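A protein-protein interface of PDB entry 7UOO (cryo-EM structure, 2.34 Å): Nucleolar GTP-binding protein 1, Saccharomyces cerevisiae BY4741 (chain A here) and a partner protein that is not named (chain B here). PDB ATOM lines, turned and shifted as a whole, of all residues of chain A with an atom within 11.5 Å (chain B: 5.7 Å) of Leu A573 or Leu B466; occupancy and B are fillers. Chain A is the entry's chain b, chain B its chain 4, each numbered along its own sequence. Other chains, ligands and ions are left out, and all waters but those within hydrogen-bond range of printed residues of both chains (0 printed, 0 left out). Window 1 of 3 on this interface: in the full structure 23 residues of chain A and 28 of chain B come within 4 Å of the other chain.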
ATOM      1  N   SER A 563      18.701  16.122  33.971  1.00  0.00           N
ATOM      2  CA  SER A 563      19.606  17.098  33.374  1.00  0.00           C
ATOM      3  C   SER A 563      20.878  17.241  34.201  1.00  0.00           C
ATOM      4  O   SER A 563      21.975  17.359  33.646  1.00  0.00           O
ATOM      5  CB  SER A 563      18.901  18.445  33.214  1.00  0.00           C
ATOM      6  OG  SER A 563      18.490  18.966  34.465  1.00  0.00           O
ATOM      7  N   VAL A 566      22.971  13.990  33.488  1.00  0.00           N
ATOM      8  CA  VAL A 566      23.543  13.838  32.153  1.00  0.00           C
ATOM      9  C   VAL A 566      24.438  15.020  31.796  1.00  0.00           C
ATOM     10  O   VAL A 566      25.629  14.845  31.518  1.00  0.00           O
ATOM     11  CB  VAL A 566      22.436  13.654  31.098  1.00  0.00           C
ATOM     12  CG1 VAL A 566      23.039  13.563  29.708  1.00  0.00           C
ATOM     13  CG2 VAL A 566      21.617  12.412  31.401  1.00  0.00           C
ATOM     14  N   PHE A 567      23.876  16.229  31.790  1.00  0.00           N
ATOM     15  CA  PHE A 567      24.584  17.423  31.349  1.00  0.00           C
ATOM     16  C   PHE A 567      25.189  18.212  32.506  1.00  0.00           C
ATOM     17  O   PHE A 567      25.497  19.396  32.341  1.00  0.00           O
ATOM     18  CB  PHE A 567      23.647  18.325  30.542  1.00  0.00           C
ATOM     19  CG  PHE A 567      23.101  17.682  29.304  1.00  0.00           C
ATOM     20  CD1 PHE A 567      23.798  17.751  28.109  1.00  0.00           C
ATOM     21  CD2 PHE A 567      21.889  17.013  29.329  1.00  0.00           C
ATOM     22  CE1 PHE A 567      23.299  17.162  26.965  1.00  0.00           C
ATOM     23  CE2 PHE A 567      21.385  16.422  28.187  1.00  0.00           C
ATOM     24  CZ  PHE A 567      22.093  16.498  27.004  1.00  0.00           C
ATOM     25  N   GLY A 568      25.359  17.582  33.669  1.00  0.00           N
ATOM     26  CA  GLY A 568      25.793  18.322  34.846  1.00  0.00           C
ATOM     27  C   GLY A 568      27.205  18.868  34.734  1.00  0.00           C
ATOM     28  O   GLY A 568      27.462  20.021  35.086  1.00  0.00           O
ATOM     29  N   ASP A 569      28.134  18.053  34.241  1.00  0.00           N
ATOM     30  CA  ASP A 569      29.532  18.451  34.141  1.00  0.00           C
ATOM     31  C   ASP A 569      29.969  18.781  32.720  1.00  0.00           C
ATOM     32  O   ASP A 569      30.993  19.449  32.545  1.00  0.00           O
ATOM     33  CB  ASP A 569      30.433  17.342  34.698  1.00  0.00           C
ATOM     34  CG  ASP A 569      30.040  15.965  34.195  1.00  0.00           C
ATOM     35  OD1 ASP A 569      29.097  15.875  33.381  1.00  0.00           O
ATOM     36  OD2 ASP A 569      30.671  14.972  34.615  1.00  0.00           O
ATOM     37  N   GLN A 570      29.222  18.341  31.712  1.00  0.00           N
ATOM     38  CA  GLN A 570      29.622  18.515  30.327  1.00  0.00           C
ATOM     39  C   GLN A 570      29.373  19.948  29.866  1.00  0.00           C
ATOM     40  O   GLN A 570      28.873  20.799  30.606  1.00  0.00           O
ATOM     41  CB  GLN A 570      28.882  17.521  29.436  1.00  0.00           C
ATOM     42  CG  GLN A 570      29.177  16.072  29.761  1.00  0.00           C
ATOM     43  CD  GLN A 570      28.392  15.113  28.898  1.00  0.00           C
ATOM     44  OE1 GLN A 570      27.557  15.524  28.093  1.00  0.00           O
ATOM     45  NE2 GLN A 570      28.656  13.823  29.059  1.00  0.00           N
ATOM     46  N   ASP A 571      29.733  20.215  28.616  1.00  0.00           N
ATOM     47  CA  ASP A 571      29.515  21.513  27.997  1.00  0.00           C
ATOM     48  C   ASP A 571      29.383  21.300  26.493  1.00  0.00           C
ATOM     49  O   ASP A 571      29.224  20.169  26.025  1.00  0.00           O
ATOM     50  CB  ASP A 571      30.653  22.477  28.356  1.00  0.00           C
ATOM     51  CG  ASP A 571      30.189  23.918  28.459  1.00  0.00           C
ATOM     52  OD1 ASP A 571      29.307  24.321  27.673  1.00  0.00           O
ATOM     53  OD2 ASP A 571      30.706  24.644  29.332  1.00  0.00           O
ATOM     54  N   ALA A 572      29.436  22.403  25.743  1.00  0.00           N
ATOM     55  CA  ALA A 572      29.509  22.400  24.284  1.00  0.00           C
ATOM     56  C   ALA A 572      28.327  21.698  23.627  1.00  0.00           C
ATOM     57  O   ALA A 572      27.239  22.275  23.535  1.00  0.00           O
ATOM     58  CB  ALA A 572      30.822  21.767  23.811  1.00  0.00           C
ATOM     59  N   LEU A 573      28.564  20.474  23.132  1.00  0.00           N
ATOM     60  CA  LEU A 573      27.660  19.662  22.311  1.00  0.00           C
ATOM     61  C   LEU A 573      27.495  20.259  20.915  1.00  0.00           C
ATOM     62  O   LEU A 573      26.844  19.667  20.048  1.00  0.00           O
ATOM     63  CB  LEU A 573      26.295  19.472  22.990  1.00  0.00           C
ATOM     64  CG  LEU A 573      25.454  18.277  22.536  1.00  0.00           C
ATOM     65  CD1 LEU A 573      26.311  17.038  22.566  1.00  0.00           C
ATOM     66  CD2 LEU A 573      24.226  18.094  23.410  1.00  0.00           C
ATOM     67  N   THR A 574      28.110  21.412  20.677  1.00  0.00           N
ATOM     68  CA  THR A 574      28.020  22.114  19.409  1.00  0.00           C
ATOM     69  C   THR A 574      29.405  22.618  19.038  1.00  0.00           C
ATOM     70  O   THR A 574      30.127  23.145  19.890  1.00  0.00           O
ATOM     71  CB  THR A 574      27.020  23.281  19.493  1.00  0.00           C
ATOM     72  OG1 THR A 574      25.684  22.766  19.519  1.00  0.00           O
ATOM     73  CG2 THR A 574      27.170  24.228  18.313  1.00  0.00           C
ATOM     74  N   ALA A 575      29.783  22.424  17.774  1.00  0.00           N
ATOM     75  CA  ALA A 575      31.031  22.974  17.264  1.00  0.00           C
ATOM     76  C   ALA A 575      31.001  24.494  17.330  1.00  0.00           C
ATOM     77  O   ALA A 575      30.239  25.135  16.599  1.00  0.00           O
ATOM     78  CB  ALA A 575      31.277  22.507  15.829  1.00  0.00           C
ATOM     79  N   SER A 576      31.816  25.078  18.207  1.00  0.00           N
ATOM     80  CA  SER A 576      31.851  26.528  18.354  1.00  0.00           C
ATOM     81  C   SER A 576      32.462  27.155  17.108  1.00  0.00           C
ATOM     82  O   SER A 576      33.588  26.821  16.723  1.00  0.00           O
ATOM     83  CB  SER A 576      32.642  26.919  19.599  1.00  0.00           C
ATOM     84  OG  SER A 576      34.014  26.592  19.458  1.00  0.00           O
ATOM     85  N   THR A 577      31.716  28.058  16.480  1.00  0.00           N
ATOM     86  CA  THR A 577      32.152  28.673  15.236  1.00  0.00           C
ATOM     87  C   THR A 577      33.304  29.640  15.479  1.00  0.00           C
ATOM     88  O   THR A 577      33.473  30.183  16.574  1.00  0.00           O
ATOM     89  CB  THR A 577      30.990  29.407  14.569  1.00  0.00           C
ATOM     90  OG1 THR A 577      30.465  30.386  15.473  1.00  0.00           O
ATOM     91  CG2 THR A 577      29.887  28.429  14.198  1.00  0.00           C
ATOM     92  N   GLU A 578      34.109  29.848  14.435  1.00  0.00           N
ATOM     93  CA  GLU A 578      35.257  30.740  14.541  1.00  0.00           C
ATOM     94  C   GLU A 578      34.856  32.208  14.583  1.00  0.00           C
ATOM     95  O   GLU A 578      35.628  33.029  15.089  1.00  0.00           O
ATOM     96  CB  GLU A 578      36.223  30.504  13.376  1.00  0.00           C
ATOM     97  CG  GLU A 578      36.935  29.160  13.403  1.00  0.00           C
ATOM     98  CD  GLU A 578      36.149  28.058  12.715  1.00  0.00           C
ATOM     99  OE1 GLU A 578      35.441  28.356  11.730  1.00  0.00           O
ATOM    100  OE2 GLU A 578      36.238  26.895  13.161  1.00  0.00           O
ATOM    101  N   LYS A 582      25.449  32.478  14.215  1.00  0.00           N
ATOM    102  CA  LYS A 582      24.311  31.621  14.509  1.00  0.00           C
ATOM    103  C   LYS A 582      24.256  30.467  13.509  1.00  0.00           C
ATOM    104  O   LYS A 582      25.055  30.384  12.573  1.00  0.00           O
ATOM    105  CB  LYS A 582      23.015  32.427  14.491  1.00  0.00           C
ATOM    106  CG  LYS A 582      22.839  33.369  15.671  1.00  0.00           C
ATOM    107  CD  LYS A 582      21.487  34.061  15.622  1.00  0.00           C
ATOM    108  CE  LYS A 582      21.199  34.837  16.900  1.00  0.00           C
ATOM    109  NZ  LYS A 582      22.067  36.037  17.055  1.00  0.00           N
ATOM    110  N   LEU A 583      23.295  29.561  13.715  1.00  0.00           N
ATOM    111  CA  LEU A 583      23.217  28.350  12.900  1.00  0.00           C
ATOM    112  C   LEU A 583      22.950  28.668  11.433  1.00  0.00           C
ATOM    113  O   LEU A 583      23.576  28.085  10.542  1.00  0.00           O
ATOM    114  CB  LEU A 583      22.134  27.420  13.448  1.00  0.00           C
ATOM    115  CG  LEU A 583      21.834  26.157  12.635  1.00  0.00           C
ATOM    116  CD1 LEU A 583      23.038  25.230  12.610  1.00  0.00           C
ATOM    117  CD2 LEU A 583      20.610  25.439  13.180  1.00  0.00           C
ATOM    118  N   ALA A 594      35.439  24.084   3.124  1.00  0.00           N
ATOM    119  CA  ALA A 594      34.628  23.154   3.903  1.00  0.00           C
ATOM    120  C   ALA A 594      35.379  22.568   5.096  1.00  0.00           C
ATOM    121  O   ALA A 594      34.794  22.407   6.172  1.00  0.00           O
ATOM    122  CB  ALA A 594      34.114  22.031   3.003  1.00  0.00           C
ATOM    123  N   GLY B 257      25.194   8.767  19.647  1.00  0.00           N
ATOM    124  CA  GLY B 257      26.083   9.466  18.745  1.00  0.00           C
ATOM    125  C   GLY B 257      26.051  10.969  18.859  1.00  0.00           C
ATOM    126  O   GLY B 257      26.812  11.654  18.170  1.00  0.00           O
ATOM    127  N   ILE B 258      25.188  11.506  19.716  1.00  0.00           N
ATOM    128  CA  ILE B 258      25.043  12.946  19.904  1.00  0.00           C
ATOM    129  C   ILE B 258      25.649  13.394  21.231  1.00  0.00           C
ATOM    130  O   ILE B 258      26.616  14.156  21.253  1.00  0.00           O
ATOM    131  CB  ILE B 258      23.561  13.371  19.791  1.00  0.00           C
ATOM    132  CG1 ILE B 258      23.023  13.041  18.398  1.00  0.00           C
ATOM    133  CG2 ILE B 258      23.401  14.850  20.105  1.00  0.00           C
ATOM    134  CD1 ILE B 258      21.583  13.437  18.188  1.00  0.00           C
ATOM    135  N   VAL B 259      25.114  12.906  22.347  1.00  0.00           N
ATOM    136  CA  VAL B 259      25.553  13.328  23.674  1.00  0.00           C
ATOM    137  C   VAL B 259      26.699  12.435  24.131  1.00  0.00           C
ATOM    138  O   VAL B 259      26.587  11.204  24.115  1.00  0.00           O
ATOM    139  CB  VAL B 259      24.387  13.283  24.677  1.00  0.00           C
ATOM    140  CG1 VAL B 259      24.834  13.797  26.037  1.00  0.00           C
ATOM    141  CG2 VAL B 259      23.207  14.090  24.160  1.00  0.00           C
ATOM    142  N   ALA B 260      27.804  13.056  24.535  1.00  0.00           N
ATOM    143  CA  ALA B 260      28.952  12.314  25.034  1.00  0.00           C
ATOM    144  C   ALA B 260      28.698  11.805  26.450  1.00  0.00           C
ATOM    145  O   ALA B 260      28.030  12.455  27.257  1.00  0.00           O
ATOM    146  CB  ALA B 260      30.203  13.189  25.010  1.00  0.00           C
ATOM    147  N   VAL B 361      16.854  16.798  20.331  1.00  0.00           N
ATOM    148  CA  VAL B 361      17.553  16.592  21.594  1.00  0.00           C
ATOM    149  C   VAL B 361      17.863  17.956  22.191  1.00  0.00           C
ATOM    150  O   VAL B 361      18.392  18.834  21.500  1.00  0.00           O
ATOM    151  CB  VAL B 361      18.841  15.770  21.403  1.00  0.00           C
ATOM    152  CG1 VAL B 361      19.595  15.641  22.719  1.00  0.00           C
ATOM    153  CG2 VAL B 361      18.517  14.399  20.835  1.00  0.00           C
ATOM    154  N   ARG B 362      17.537  18.131  23.470  1.00  0.00           N
ATOM    155  CA  ARG B 362      17.796  19.377  24.180  1.00  0.00           C
ATOM    156  C   ARG B 362      19.188  19.348  24.800  1.00  0.00           C
ATOM    157  O   ARG B 362      19.565  18.370  25.452  1.00  0.00           O
ATOM    158  CB  ARG B 362      16.739  19.606  25.262  1.00  0.00           C
ATOM    159  CG  ARG B 362      17.072  20.709  26.260  1.00  0.00           C
ATOM    160  CD  ARG B 362      16.814  22.095  25.694  1.00  0.00           C
ATOM    161  NE  ARG B 362      16.888  23.124  26.724  1.00  0.00           N
ATOM    162  CZ  ARG B 362      17.938  23.907  26.932  1.00  0.00           C
ATOM    163  NH1 ARG B 362      19.025  23.822  26.183  1.00  0.00           N
ATOM    164  NH2 ARG B 362      17.897  24.799  27.916  1.00  0.00           N
ATOM    165  N   ASP B 363      19.947  20.422  24.590  1.00  0.00           N
ATOM    166  CA  ASP B 363      21.291  20.576  25.146  1.00  0.00           C
ATOM    167  C   ASP B 363      21.188  21.454  26.388  1.00  0.00           C
ATOM    168  O   ASP B 363      21.096  22.679  26.289  1.00  0.00           O
ATOM    169  CB  ASP B 363      22.231  21.180  24.108  1.00  0.00           C
ATOM    170  CG  ASP B 363      23.655  21.319  24.611  1.00  0.00           C
ATOM    171  OD1 ASP B 363      23.999  20.696  25.638  1.00  0.00           O
ATOM    172  OD2 ASP B 363      24.433  22.054  23.972  1.00  0.00           O
ATOM    173  N   VAL B 433      19.268  20.252  19.177  1.00  0.00           N
ATOM    174  CA  VAL B 433      19.823  19.700  17.951  1.00  0.00           C
ATOM    175  C   VAL B 433      18.916  18.579  17.460  1.00  0.00           C
ATOM    176  O   VAL B 433      18.065  18.066  18.189  1.00  0.00           O
ATOM    177  CB  VAL B 433      21.266  19.189  18.136  1.00  0.00           C
ATOM    178  CG1 VAL B 433      22.183  20.329  18.546  1.00  0.00           C
ATOM    179  CG2 VAL B 433      21.307  18.072  19.162  1.00  0.00           C
ATOM    180  N   GLU B 434      19.112  18.202  16.202  1.00  0.00           N
ATOM    181  CA  GLU B 434      18.318  17.172  15.550  1.00  0.00           C
ATOM    182  C   GLU B 434      19.012  15.818  15.636  1.00  0.00           C
ATOM    183  O   GLU B 434      20.242  15.727  15.623  1.00  0.00           O
ATOM    184  CB  GLU B 434      18.074  17.520  14.082  1.00  0.00           C
ATOM    185  CG  GLU B 434      17.276  18.787  13.850  1.00  0.00           C
ATOM    186  CD  GLU B 434      17.207  19.161  12.382  1.00  0.00           C
ATOM    187  OE1 GLU B 434      18.155  18.827  11.641  1.00  0.00           O
ATOM    188  OE2 GLU B 434      16.205  19.781  11.968  1.00  0.00           O
ATOM    189  N   SER B 464      30.165  21.258  10.368  1.00  0.00           N
ATOM    190  CA  SER B 464      29.264  20.374  11.093  1.00  0.00           C
ATOM    191  C   SER B 464      28.832  21.018  12.404  1.00  0.00           C
ATOM    192  O   SER B 464      29.669  21.480  13.185  1.00  0.00           O
ATOM    193  CB  SER B 464      29.948  19.033  11.359  1.00  0.00           C
ATOM    194  OG  SER B 464      29.150  18.203  12.182  1.00  0.00           O
ATOM    195  N   THR B 465      27.520  21.051  12.643  1.00  0.00           N
ATOM    196  CA  THR B 465      27.010  21.647  13.874  1.00  0.00           C
ATOM    197  C   THR B 465      27.314  20.773  15.087  1.00  0.00           C
ATOM    198  O   THR B 465      27.684  21.285  16.149  1.00  0.00           O
ATOM    199  CB  THR B 465      25.505  21.906  13.753  1.00  0.00           C
ATOM    200  OG1 THR B 465      24.821  20.674  13.492  1.00  0.00           O
ATOM    201  CG2 THR B 465      25.210  22.904  12.641  1.00  0.00           C
ATOM    202  N   LEU B 466      27.173  19.457  14.950  1.00  0.00           N
ATOM    203  CA  LEU B 466      27.418  18.551  16.064  1.00  0.00           C
ATOM    204  C   LEU B 466      28.908  18.280  16.223  1.00  0.00           C
ATOM    205  O   LEU B 466      29.622  18.053  15.242  1.00  0.00           O
ATOM    206  CB  LEU B 466      26.660  17.240  15.860  1.00  0.00           C
ATOM    207  CG  LEU B 466      25.337  17.073  16.610  1.00  0.00           C
ATOM    208  CD1 LEU B 466      25.573  17.111  18.108  1.00  0.00           C
ATOM    209  CD2 LEU B 466      24.337  18.139  16.197  1.00  0.00           C
ATOM    210  N   THR B 467      29.373  18.303  17.473  1.00  0.00           N
ATOM    211  CA  THR B 467      30.796  18.124  17.751  1.00  0.00           C
ATOM    212  C   THR B 467      31.250  16.696  17.464  1.00  0.00           C
ATOM    213  O   THR B 467      32.262  16.484  16.785  1.00  0.00           O
ATOM    214  CB  THR B 467      31.094  18.499  19.207  1.00  0.00           C
ATOM    215  OG1 THR B 467      31.014  19.920  19.366  1.00  0.00           O
ATOM    216  CG2 THR B 467      32.482  18.029  19.615  1.00  0.00           C
ATOM    217  N   LEU B 468      30.511  15.705  17.969  1.00  0.00           N
ATOM    218  CA  LEU B 468      30.976  14.318  17.908  1.00  0.00           C
ATOM    219  C   LEU B 468      31.128  13.779  16.485  1.00  0.00           C
ATOM    220  O   LEU B 468      32.187  13.199  16.187  1.00  0.00           O
ATOM    221  CB  LEU B 468      30.060  13.428  18.760  1.00  0.00           C
ATOM    222  CG  LEU B 468      30.448  13.164  20.219  1.00  0.00           C
ATOM    223  CD1 LEU B 468      30.505  14.449  21.028  1.00  0.00           C
ATOM    224  CD2 LEU B 468      29.481  12.172  20.852  1.00  0.00           C
ATOM    225  N   PRO B 469      30.158  13.919  15.566  1.00  0.00           N
ATOM    226  CA  PRO B 469      30.402  13.434  14.198  1.00  0.00           C
ATOM    227  C   PRO B 469      31.294  14.341  13.366  1.00  0.00           C
ATOM    228  O   PRO B 469      31.808  13.887  12.336  1.00  0.00           O
ATOM    229  CB  PRO B 469      28.992  13.352  13.588  1.00  0.00           C
ATOM    230  CG  PRO B 469      28.050  13.467  14.740  1.00  0.00           C
ATOM    231  CD  PRO B 469      28.753  14.337  15.718  1.00  0.00           C
ATOM    232  N   GLY B 470      31.482  15.600  13.767  1.00  0.00           N
ATOM    233  CA  GLY B 470      32.312  16.502  12.984  1.00  0.00           C
ATOM    234  C   GLY B 470      33.776  16.107  12.977  1.00  0.00           C
ATOM    235  O   GLY B 470      34.434  16.146  11.933  1.00  0.00           O
ATOM    236  N   HIS B 471      34.308  15.726  14.135  1.00  0.00           N
ATOM    237  CA  HIS B 471      35.699  15.302  14.278  1.00  0.00           C
ATOM    238  C   HIS B 471      35.692  13.784  14.424  1.00  0.00           C
ATOM    239  O   HIS B 471      35.547  13.258  15.530  1.00  0.00           O
ATOM    240  CB  HIS B 471      36.356  15.985  15.475  1.00  0.00           C
ATOM    241  CG  HIS B 471      37.833  16.186  15.325  1.00  0.00           C
ATOM    242  ND1 HIS B 471      38.762  15.405  15.976  1.00  0.00           N
ATOM    243  CD2 HIS B 471      38.539  17.086  14.600  1.00  0.00           C
ATOM    244  CE1 HIS B 471      39.978  15.813  15.659  1.00  0.00           C
ATOM    245  NE2 HIS B 471      39.870  16.832  14.824  1.00  0.00           N
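The side-chain amide oxygen of Gln A570 lies close to the backbone carbonyl oxygen of Ala B260.
The side-chain hydroxyl (OG1) of Thr B467 sits close to the backbone carbonyl oxygen (O) of Thr A574, 3.4 Å away.
The backbone NH (N) of Ala A575 lies within hydrogen-bond range of the backbone carbonyl oxygen (O) of Thr B465 (2.9 Å).
The side-chain hydroxyl of Thr B467 sits at hydrogen-bond distance from the backbone NH of Ala A575, at 3.2 Å.
The backbone carbonyl oxygen of Ala A572 sits close to the side-chain carboxylate of Asp B363 (2.8 Å).
O of Leu B466 is in hydrogen-bond range of OG of Ser B464 (3.1 Å).
Among the printed residues, pairs that only touch across the chains: Phe A567 with Val B259 (3.8 Å), Phe A567 with Arg B362 (3.5 Å), Phe A567 with Asp B363 (3.8 Å), Gln A570 with Val B259 (3.8 Å), Leu A573 with Ile B258 (3.2 Å), Leu A573 with Val B259 (3.9 Å), Leu A573 with Asp B363 (3.3 Å), Leu A573 with Leu B466 (3.5 Å), Leu A573 with Thr B467 (3.9 Å), Thr A574 with Thr B465 (3.4 Å), Ala A575 with Ser B464 (3.3 Å) and Leu A583 with Thr B465 (3.2 Å).
Asp A571 touches none of the printed residues of chain B.
Leu A573 touches just these residues of chain B: Ile B258, Val B259, Asp B363, Leu B466 and Thr B467.
Printed residues of chain B within 4 Å of Leu A583: Thr B465.
Gly B257 touches none of the printed residues of chain A.
Ile B258 touches just one residue of chain A: Leu A573 (3.2 Å).
Of the printed residues of chain A, Arg B362 touches Phe A567.
Val B433 touches none of the printed residues of chain A.
Ser B464 touches one residue of chain A.
No residue of chain A comes within 4 Å of Leu B468.
No residue of chain A comes within 4 Å of Gly B470.
The nearest printed residue of chain A that does not touch Arg B362 is Leu A573 (5.1 Å).
Hydrophobic or aromatic side chains of chain A within 4 Å of the printed part of chain B: Phe A567, Leu A573, Ala A575 and Leu A583.
Along chain A the printed residues that touch a printed residue of chain B span positions 567 to 583.
Of the 17 printed residues of chain B, 9 touch a printed residue of chain A.
Printed residues of chain B that touch a printed residue of chain A: Ile B258, Val B259, Ala B260, Arg B362, Asp B363, Ser B464, Thr B465, Leu B466 and Thr B467.
Hydrophobic or aromatic side chains of chain B within 4 Å of the printed part of chain A: Val B259 and Leu B466.
Among the printed residues, 17 pairs touch across the chains.
Among the printed residues, no Asp or Glu carboxylate lies within 4 Å of a Lys or Arg side-chain nitrogen of the other chain.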
